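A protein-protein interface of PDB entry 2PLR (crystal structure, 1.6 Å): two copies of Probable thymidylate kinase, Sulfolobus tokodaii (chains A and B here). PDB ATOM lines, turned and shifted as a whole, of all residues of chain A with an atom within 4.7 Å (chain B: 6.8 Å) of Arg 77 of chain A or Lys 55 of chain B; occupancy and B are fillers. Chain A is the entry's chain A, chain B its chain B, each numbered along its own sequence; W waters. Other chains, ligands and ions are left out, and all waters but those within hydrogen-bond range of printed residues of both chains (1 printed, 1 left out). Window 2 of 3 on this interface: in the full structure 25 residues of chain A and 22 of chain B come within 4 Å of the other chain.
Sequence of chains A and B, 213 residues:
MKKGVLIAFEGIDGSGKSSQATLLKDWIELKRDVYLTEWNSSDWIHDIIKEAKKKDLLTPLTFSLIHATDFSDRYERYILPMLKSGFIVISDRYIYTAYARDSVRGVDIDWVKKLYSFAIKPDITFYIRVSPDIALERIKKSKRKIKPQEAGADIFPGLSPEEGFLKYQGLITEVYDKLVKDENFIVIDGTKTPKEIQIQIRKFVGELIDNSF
The backbone carbonyl oxygen (O) of Lys 55 of chain B is in hydrogen-bond range of the guanidinium group (NH2) of Arg 77 of chain A (3.1 Å).
The backbone carbonyl oxygen (O) of Leu 57 of chain B lies within hydrogen-bond range of the guanidinium group (NH1) of Arg 77 of chain A.
The indole nitrogen (NE1) of Trp 44 of chain A is in hydrogen-bond range of the side-chain carboxylate (OD1) of Asp 73 of chain A (3.0 Å).
NE of Arg 77 of chain A is in salt-bridge range of OD1 of Asp 73 of chain A.
The side-chain carboxylate (OE1) of Glu 51 of chain B lies within salt-bridge range of the side-chain amino group (NZ) of Lys 54 of chain B, at 3.7 Å.
The side-chain carboxylate (OE2) of Glu 51 of chain B lies within salt-bridge range of the side-chain amino group (NZ) of Lys 55 of chain B (3.8 Å).
N of Leu 57 of chain B sits at hydrogen-bond distance from O of Ala 52 of chain B, 3.3 Å away.
Among the printed residues, merely in contact across the chains: Trp 44 of chain A with Glu 51 of chain B, Trp 44 of chain A with Ala 52 of chain B, Trp 44 of chain A with Lys 55 of chain B and Glu 76 of chain A with Thr 59 of chain B.
Lys 55 of chain B touches two residues of chain A.
Of the printed residues of chain A, Leu 57 of chain B touches Arg 77.
Of the printed residues of chain A, Glu 51 of chain B touches Trp 44.
Of the printed residues of chain B, Trp 44 of chain A touches Glu 51, Ala 52 and Lys 55.
Of the printed residues of chain B, Glu 76 of chain A touches Thr 59.
The nearest residue of chain B that does not touch Arg 77 of chain A is Leu 58 of chain B (4.9 Å).
Printed residues of chain B that touch a printed residue of chain A: Glu 51, Ala 52, Lys 55, Leu 57 and Thr 59.
Hydrophobic or aromatic side chains of chain B within 4 Å of the printed part of chain A: Ala 52 and Leu 57.
Hydrophobic or aromatic side chains of chain A that line the printed part of chain B: Trp 44.
Among the printed residues, 6 pairs touch across the chains.
Among the printed residues, no Asp or Glu carboxylate lies within 4 Å of a Lys or Arg side-chain nitrogen of the other chain.
No position is printed for both chains.
Water W1 lies within hydrogen-bond range of OD2 of Asp 73 of chain A (2.8 Å) and N of Thr 59 of chain B (3.0 Å).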
ATOM      1  N   TRP A  44     -10.078  -5.779  27.415  1.00  0.00           N
ATOM      2  CA  TRP A  44     -10.619  -6.395  28.623  1.00  0.00           C
ATOM      3  C   TRP A  44     -12.124  -6.585  28.776  1.00  0.00           C
ATOM      4  O   TRP A  44     -12.555  -7.602  29.317  1.00  0.00           O
ATOM      5  CB  TRP A  44     -10.066  -5.674  29.857  1.00  0.00           C
ATOM      6  CG  TRP A  44     -10.511  -4.262  29.986  1.00  0.00           C
ATOM      7  CD1 TRP A  44     -10.029  -3.181  29.307  1.00  0.00           C
ATOM      8  CD2 TRP A  44     -11.559  -3.776  30.828  1.00  0.00           C
ATOM      9  NE1 TRP A  44     -10.714  -2.048  29.675  1.00  0.00           N
ATOM     10  CE2 TRP A  44     -11.658  -2.384  30.608  1.00  0.00           C
ATOM     11  CE3 TRP A  44     -12.424  -4.379  31.751  1.00  0.00           C
ATOM     12  CZ2 TRP A  44     -12.593  -1.586  31.276  1.00  0.00           C
ATOM     13  CZ3 TRP A  44     -13.352  -3.584  32.415  1.00  0.00           C
ATOM     14  CH2 TRP A  44     -13.427  -2.202  32.174  1.00  0.00           C
ATOM     15  N   ASP A  73     -14.458   1.495  24.609  1.00  0.00           N
ATOM     16  CA  ASP A  73     -13.445   1.697  25.642  1.00  0.00           C
ATOM     17  C   ASP A  73     -12.073   1.897  24.993  1.00  0.00           C
ATOM     18  O   ASP A  73     -11.324   2.797  25.367  1.00  0.00           O
ATOM     19  CB  ASP A  73     -13.402   0.507  26.604  1.00  0.00           C
ATOM     20  CG  ASP A  73     -12.481   0.755  27.783  1.00  0.00           C
ATOM     21  OD1 ASP A  73     -11.349   0.233  27.781  1.00  0.00           O
ATOM     22  OD2 ASP A  73     -12.887   1.491  28.705  1.00  0.00           O
ATOM     23  N   ARG A  74     -11.742   1.061  24.013  1.00  0.00           N
ATOM     24  CA  ARG A  74     -10.458   1.202  23.330  1.00  0.00           C
ATOM     25  C   ARG A  74     -10.368   2.580  22.694  1.00  0.00           C
ATOM     26  O   ARG A  74      -9.308   3.208  22.673  1.00  0.00           O
ATOM     27  CB  ARG A  74     -10.311   0.149  22.229  1.00  0.00           C
ATOM     28  CG  ARG A  74     -10.161  -1.274  22.727  1.00  0.00           C
ATOM     29  CD  ARG A  74     -10.315  -2.258  21.573  1.00  0.00           C
ATOM     30  NE  ARG A  74      -9.299  -2.048  20.548  1.00  0.00           N
ATOM     31  CZ  ARG A  74      -9.269  -2.683  19.381  1.00  0.00           C
ATOM     32  NH1 ARG A  74     -10.207  -3.572  19.077  1.00  0.00           N
ATOM     33  NH2 ARG A  74      -8.285  -2.445  18.524  1.00  0.00           N
ATOM     34  N   TYR A  75     -11.494   3.036  22.160  1.00  0.00           N
ATOM     35  CA  TYR A  75     -11.578   4.327  21.490  1.00  0.00           C
ATOM     36  C   TYR A  75     -11.267   5.501  22.420  1.00  0.00           C
ATOM     37  O   TYR A  75     -10.461   6.373  22.091  1.00  0.00           O
ATOM     38  CB  TYR A  75     -12.978   4.493  20.900  1.00  0.00           C
ATOM     39  CG  TYR A  75     -13.152   5.727  20.052  1.00  0.00           C
ATOM     40  CD1 TYR A  75     -12.507   5.849  18.821  1.00  0.00           C
ATOM     41  CD2 TYR A  75     -13.978   6.766  20.469  1.00  0.00           C
ATOM     42  CE1 TYR A  75     -12.690   6.978  18.025  1.00  0.00           C
ATOM     43  CE2 TYR A  75     -14.166   7.897  19.685  1.00  0.00           C
ATOM     44  CZ  TYR A  75     -13.521   7.997  18.466  1.00  0.00           C
ATOM     45  OH  TYR A  75     -13.723   9.111  17.688  1.00  0.00           O
ATOM     46  N   GLU A  76     -11.911   5.523  23.580  1.00  0.00           N
ATOM     47  CA  GLU A  76     -11.701   6.600  24.542  1.00  0.00           C
ATOM     48  C   GLU A  76     -10.399   6.463  25.324  1.00  0.00           C
ATOM     49  O   GLU A  76      -9.799   7.465  25.719  1.00  0.00           O
ATOM     50  CB  GLU A  76     -12.875   6.646  25.519  1.00  0.00           C
ATOM     51  CG  GLU A  76     -14.214   6.794  24.828  1.00  0.00           C
ATOM     52  CD  GLU A  76     -14.665   8.232  24.711  1.00  0.00           C
ATOM     53  OE1 GLU A  76     -13.799   9.127  24.594  1.00  0.00           O
ATOM     54  OE2 GLU A  76     -15.893   8.464  24.725  1.00  0.00           O
ATOM     55  N   ARG A  77      -9.962   5.228  25.540  1.00  0.00           N
ATOM     56  CA  ARG A  77      -8.746   4.953  26.302  1.00  0.00           C
ATOM     57  C   ARG A  77      -7.449   5.130  25.517  1.00  0.00           C
ATOM     58  O   ARG A  77      -6.482   5.701  26.030  1.00  0.00           O
ATOM     59  CB  ARG A  77      -8.810   3.527  26.865  1.00  0.00           C
ATOM     60  CG  ARG A  77      -7.715   3.164  27.866  1.00  0.00           C
ATOM     61  CD  ARG A  77      -7.879   1.724  28.356  1.00  0.00           C
ATOM     62  NE  ARG A  77      -9.168   1.505  29.013  1.00  0.00           N
ATOM     63  CZ  ARG A  77      -9.499   1.998  30.205  1.00  0.00           C
ATOM     64  NH1 ARG A  77     -10.700   1.750  30.717  1.00  0.00           N
ATOM     65  NH2 ARG A  77      -8.628   2.726  30.894  1.00  0.00           N
ATOM     66  N   TYR A  78      -7.431   4.663  24.271  1.00  0.00           N
ATOM     67  CA  TYR A  78      -6.222   4.730  23.455  1.00  0.00           C
ATOM     68  C   TYR A  78      -6.280   5.554  22.175  1.00  0.00           C
ATOM     69  O   TYR A  78      -5.499   6.487  21.983  1.00  0.00           O
ATOM     70  CB  TYR A  78      -5.789   3.311  23.074  1.00  0.00           C
ATOM     71  CG  TYR A  78      -5.516   2.408  24.249  1.00  0.00           C
ATOM     72  CD1 TYR A  78      -4.455   2.666  25.114  1.00  0.00           C
ATOM     73  CD2 TYR A  78      -6.315   1.291  24.497  1.00  0.00           C
ATOM     74  CE1 TYR A  78      -4.192   1.834  26.199  1.00  0.00           C
ATOM     75  CE2 TYR A  78      -6.062   0.451  25.582  1.00  0.00           C
ATOM     76  CZ  TYR A  78      -4.996   0.731  26.427  1.00  0.00           C
ATOM     77  OH  TYR A  78      -4.728  -0.088  27.501  1.00  0.00           O
ATOM     78  N   ILE A  79      -7.205   5.198  21.293  1.00  0.00           N
ATOM     79  CA  ILE A  79      -7.314   5.851  19.998  1.00  0.00           C
ATOM     80  C   ILE A  79      -7.567   7.352  19.956  1.00  0.00           C
ATOM     81  O   ILE A  79      -6.770   8.098  19.384  1.00  0.00           O
ATOM     82  CB  ILE A  79      -8.380   5.147  19.136  1.00  0.00           C
ATOM     83  CG1 ILE A  79      -8.014   3.672  18.978  1.00  0.00           C
ATOM     84  CG2 ILE A  79      -8.468   5.816  17.768  1.00  0.00           C
ATOM     85  CD1 ILE A  79      -9.060   2.855  18.258  1.00  0.00           C
ATOM     86  N   PRO A  81      -7.417   9.633  22.372  1.00  0.00           N
ATOM     87  CA  PRO A  81      -6.398  10.431  23.061  1.00  0.00           C
ATOM     88  C   PRO A  81      -5.159  10.638  22.190  1.00  0.00           C
ATOM     89  O   PRO A  81      -4.594  11.733  22.142  1.00  0.00           O
ATOM     90  CB  PRO A  81      -6.091   9.601  24.305  1.00  0.00           C
ATOM     91  CG  PRO A  81      -7.400   8.942  24.591  1.00  0.00           C
ATOM     92  CD  PRO A  81      -7.846   8.502  23.215  1.00  0.00           C
ATOM     93  N   LYS B  50     -15.912  -3.013  38.503  1.00  0.00           N
ATOM     94  CA  LYS B  50     -14.820  -3.197  39.450  1.00  0.00           C
ATOM     95  C   LYS B  50     -13.468  -3.112  38.742  1.00  0.00           C
ATOM     96  O   LYS B  50     -12.549  -2.443  39.216  1.00  0.00           O
ATOM     97  CB  LYS B  50     -14.959  -4.546  40.162  1.00  0.00           C
ATOM     98  CG  LYS B  50     -13.879  -4.809  41.203  1.00  0.00           C
ATOM     99  CD  LYS B  50     -14.434  -5.513  42.437  1.00  0.00           C
ATOM    100  CE  LYS B  50     -14.963  -6.904  42.123  1.00  0.00           C
ATOM    101  NZ  LYS B  50     -15.488  -7.575  43.348  1.00  0.00           N
ATOM    102  N   GLU B  51     -13.355  -3.787  37.602  1.00  0.00           N
ATOM    103  CA  GLU B  51     -12.119  -3.783  36.831  1.00  0.00           C
ATOM    104  C   GLU B  51     -11.861  -2.397  36.238  1.00  0.00           C
ATOM    105  O   GLU B  51     -10.717  -1.957  36.147  1.00  0.00           O
ATOM    106  CB  GLU B  51     -12.203  -4.832  35.714  1.00  0.00           C
ATOM    107  CG  GLU B  51     -10.891  -5.120  34.998  1.00  0.00           C
ATOM    108  CD  GLU B  51      -9.800  -5.605  35.937  1.00  0.00           C
ATOM    109  OE1 GLU B  51     -10.114  -6.353  36.887  1.00  0.00           O
ATOM    110  OE2 GLU B  51      -8.624  -5.248  35.715  1.00  0.00           O
ATOM    111  N   ALA B  52     -12.929  -1.710  35.845  1.00  0.00           N
ATOM    112  CA  ALA B  52     -12.811  -0.374  35.268  1.00  0.00           C
ATOM    113  C   ALA B  52     -12.199   0.595  36.275  1.00  0.00           C
ATOM    114  O   ALA B  52     -11.455   1.506  35.905  1.00  0.00           O
ATOM    115  CB  ALA B  52     -14.183   0.131  34.827  1.00  0.00           C
ATOM    116  N   LYS B  53     -12.523   0.401  37.549  1.00  0.00           N
ATOM    117  CA  LYS B  53     -11.988   1.258  38.601  1.00  0.00           C
ATOM    118  C   LYS B  53     -10.481   1.064  38.707  1.00  0.00           C
ATOM    119  O   LYS B  53      -9.742   2.004  38.994  1.00  0.00           O
ATOM    120  CB  LYS B  53     -12.654   0.936  39.941  1.00  0.00           C
ATOM    121  CG  LYS B  53     -14.133   1.287  39.983  1.00  0.00           C
ATOM    122  CD  LYS B  53     -14.732   1.004  41.350  1.00  0.00           C
ATOM    123  CE  LYS B  53     -16.187   1.439  41.411  1.00  0.00           C
ATOM    124  NZ  LYS B  53     -16.777   1.237  42.766  1.00  0.00           N
ATOM    125  N   LYS B  54     -10.030  -0.162  38.468  1.00  0.00           N
ATOM    126  CA  LYS B  54      -8.606  -0.462  38.525  1.00  0.00           C
ATOM    127  C   LYS B  54      -7.910   0.159  37.321  1.00  0.00           C
ATOM    128  O   LYS B  54      -6.694   0.346  37.321  1.00  0.00           O
ATOM    129  CB  LYS B  54      -8.379  -1.977  38.518  1.00  0.00           C
ATOM    130  CG  LYS B  54      -9.028  -2.720  39.674  1.00  0.00           C
ATOM    131  CD  LYS B  54      -8.796  -4.220  39.552  1.00  0.00           C
ATOM    132  CE  LYS B  54      -9.526  -4.988  40.638  1.00  0.00           C
ATOM    133  NZ  LYS B  54      -9.342  -6.461  40.486  1.00  0.00           N
ATOM    134  N   LYS B  55      -8.694   0.489  36.297  1.00  0.00           N
ATOM    135  CA  LYS B  55      -8.161   1.070  35.072  1.00  0.00           C
ATOM    136  C   LYS B  55      -8.419   2.567  34.926  1.00  0.00           C
ATOM    137  O   LYS B  55      -8.145   3.153  33.877  1.00  0.00           O
ATOM    138  CB  LYS B  55      -8.723   0.318  33.866  1.00  0.00           C
ATOM    139  CG  LYS B  55      -8.385  -1.163  33.882  1.00  0.00           C
ATOM    140  CD  LYS B  55      -8.994  -1.893  32.702  1.00  0.00           C
ATOM    141  CE  LYS B  55      -8.606  -3.364  32.716  1.00  0.00           C
ATOM    142  NZ  LYS B  55      -7.134  -3.543  32.606  1.00  0.00           N
ATOM    143  N   ASP B  56      -8.952   3.178  35.979  1.00  0.00           N
ATOM    144  CA  ASP B  56      -9.226   4.613  36.004  1.00  0.00           C
ATOM    145  C   ASP B  56     -10.115   5.195  34.916  1.00  0.00           C
ATOM    146  O   ASP B  56     -10.061   6.398  34.661  1.00  0.00           O
ATOM    147  CB  ASP B  56      -7.917   5.405  36.005  1.00  0.00           C
ATOM    148  CG  ASP B  56      -7.336   5.566  37.387  1.00  0.00           C
ATOM    149  OD1 ASP B  56      -8.104   5.478  38.368  1.00  0.00           O
ATOM    150  OD2 ASP B  56      -6.116   5.802  37.489  1.00  0.00           O
ATOM    151  N   LEU B  57     -10.937   4.375  34.276  1.00  0.00           N
ATOM    152  CA  LEU B  57     -11.796   4.914  33.236  1.00  0.00           C
ATOM    153  C   LEU B  57     -12.953   4.027  32.820  1.00  0.00           C
ATOM    154  O   LEU B  57     -12.793   2.828  32.606  1.00  0.00           O
ATOM    155  CB  LEU B  57     -10.971   5.252  31.989  1.00  0.00           C
ATOM    156  CG  LEU B  57     -11.769   5.768  30.784  1.00  0.00           C
ATOM    157  CD1 LEU B  57     -12.377   7.124  31.111  1.00  0.00           C
ATOM    158  CD2 LEU B  57     -10.863   5.869  29.568  1.00  0.00           C
ATOM    159  N   LEU B  58     -14.123   4.647  32.729  1.00  0.00           N
ATOM    160  CA  LEU B  58     -15.344   3.993  32.277  1.00  0.00           C
ATOM    161  C   LEU B  58     -16.263   5.139  31.888  1.00  0.00           C
ATOM    162  O   LEU B  58     -16.866   5.783  32.742  1.00  0.00           O
ATOM    163  CB  LEU B  58     -15.991   3.151  33.376  1.00  0.00           C
ATOM    164  CG  LEU B  58     -17.162   2.318  32.841  1.00  0.00           C
ATOM    165  CD1 LEU B  58     -16.657   1.321  31.798  1.00  0.00           C
ATOM    166  CD2 LEU B  58     -17.844   1.594  33.987  1.00  0.00           C
ATOM    167  N   THR B  59     -16.348   5.393  30.589  1.00  0.00           N
ATOM    168  CA  THR B  59     -17.157   6.482  30.060  1.00  0.00           C
ATOM    169  C   THR B  59     -18.647   6.185  30.079  1.00  0.00           C
ATOM    170  O   THR B  59     -19.061   5.024  30.121  1.00  0.00           O
ATOM    171  CB  THR B  59     -16.775   6.778  28.609  1.00  0.00           C
ATOM    172  OG1 THR B  59     -17.209   5.689  27.784  1.00  0.00           O
ATOM    173  CG2 THR B  59     -15.267   6.932  28.479  1.00  0.00           C
HETATM  174  O   HOH W   1     -14.936   3.414  28.825  1.00  0.00           O
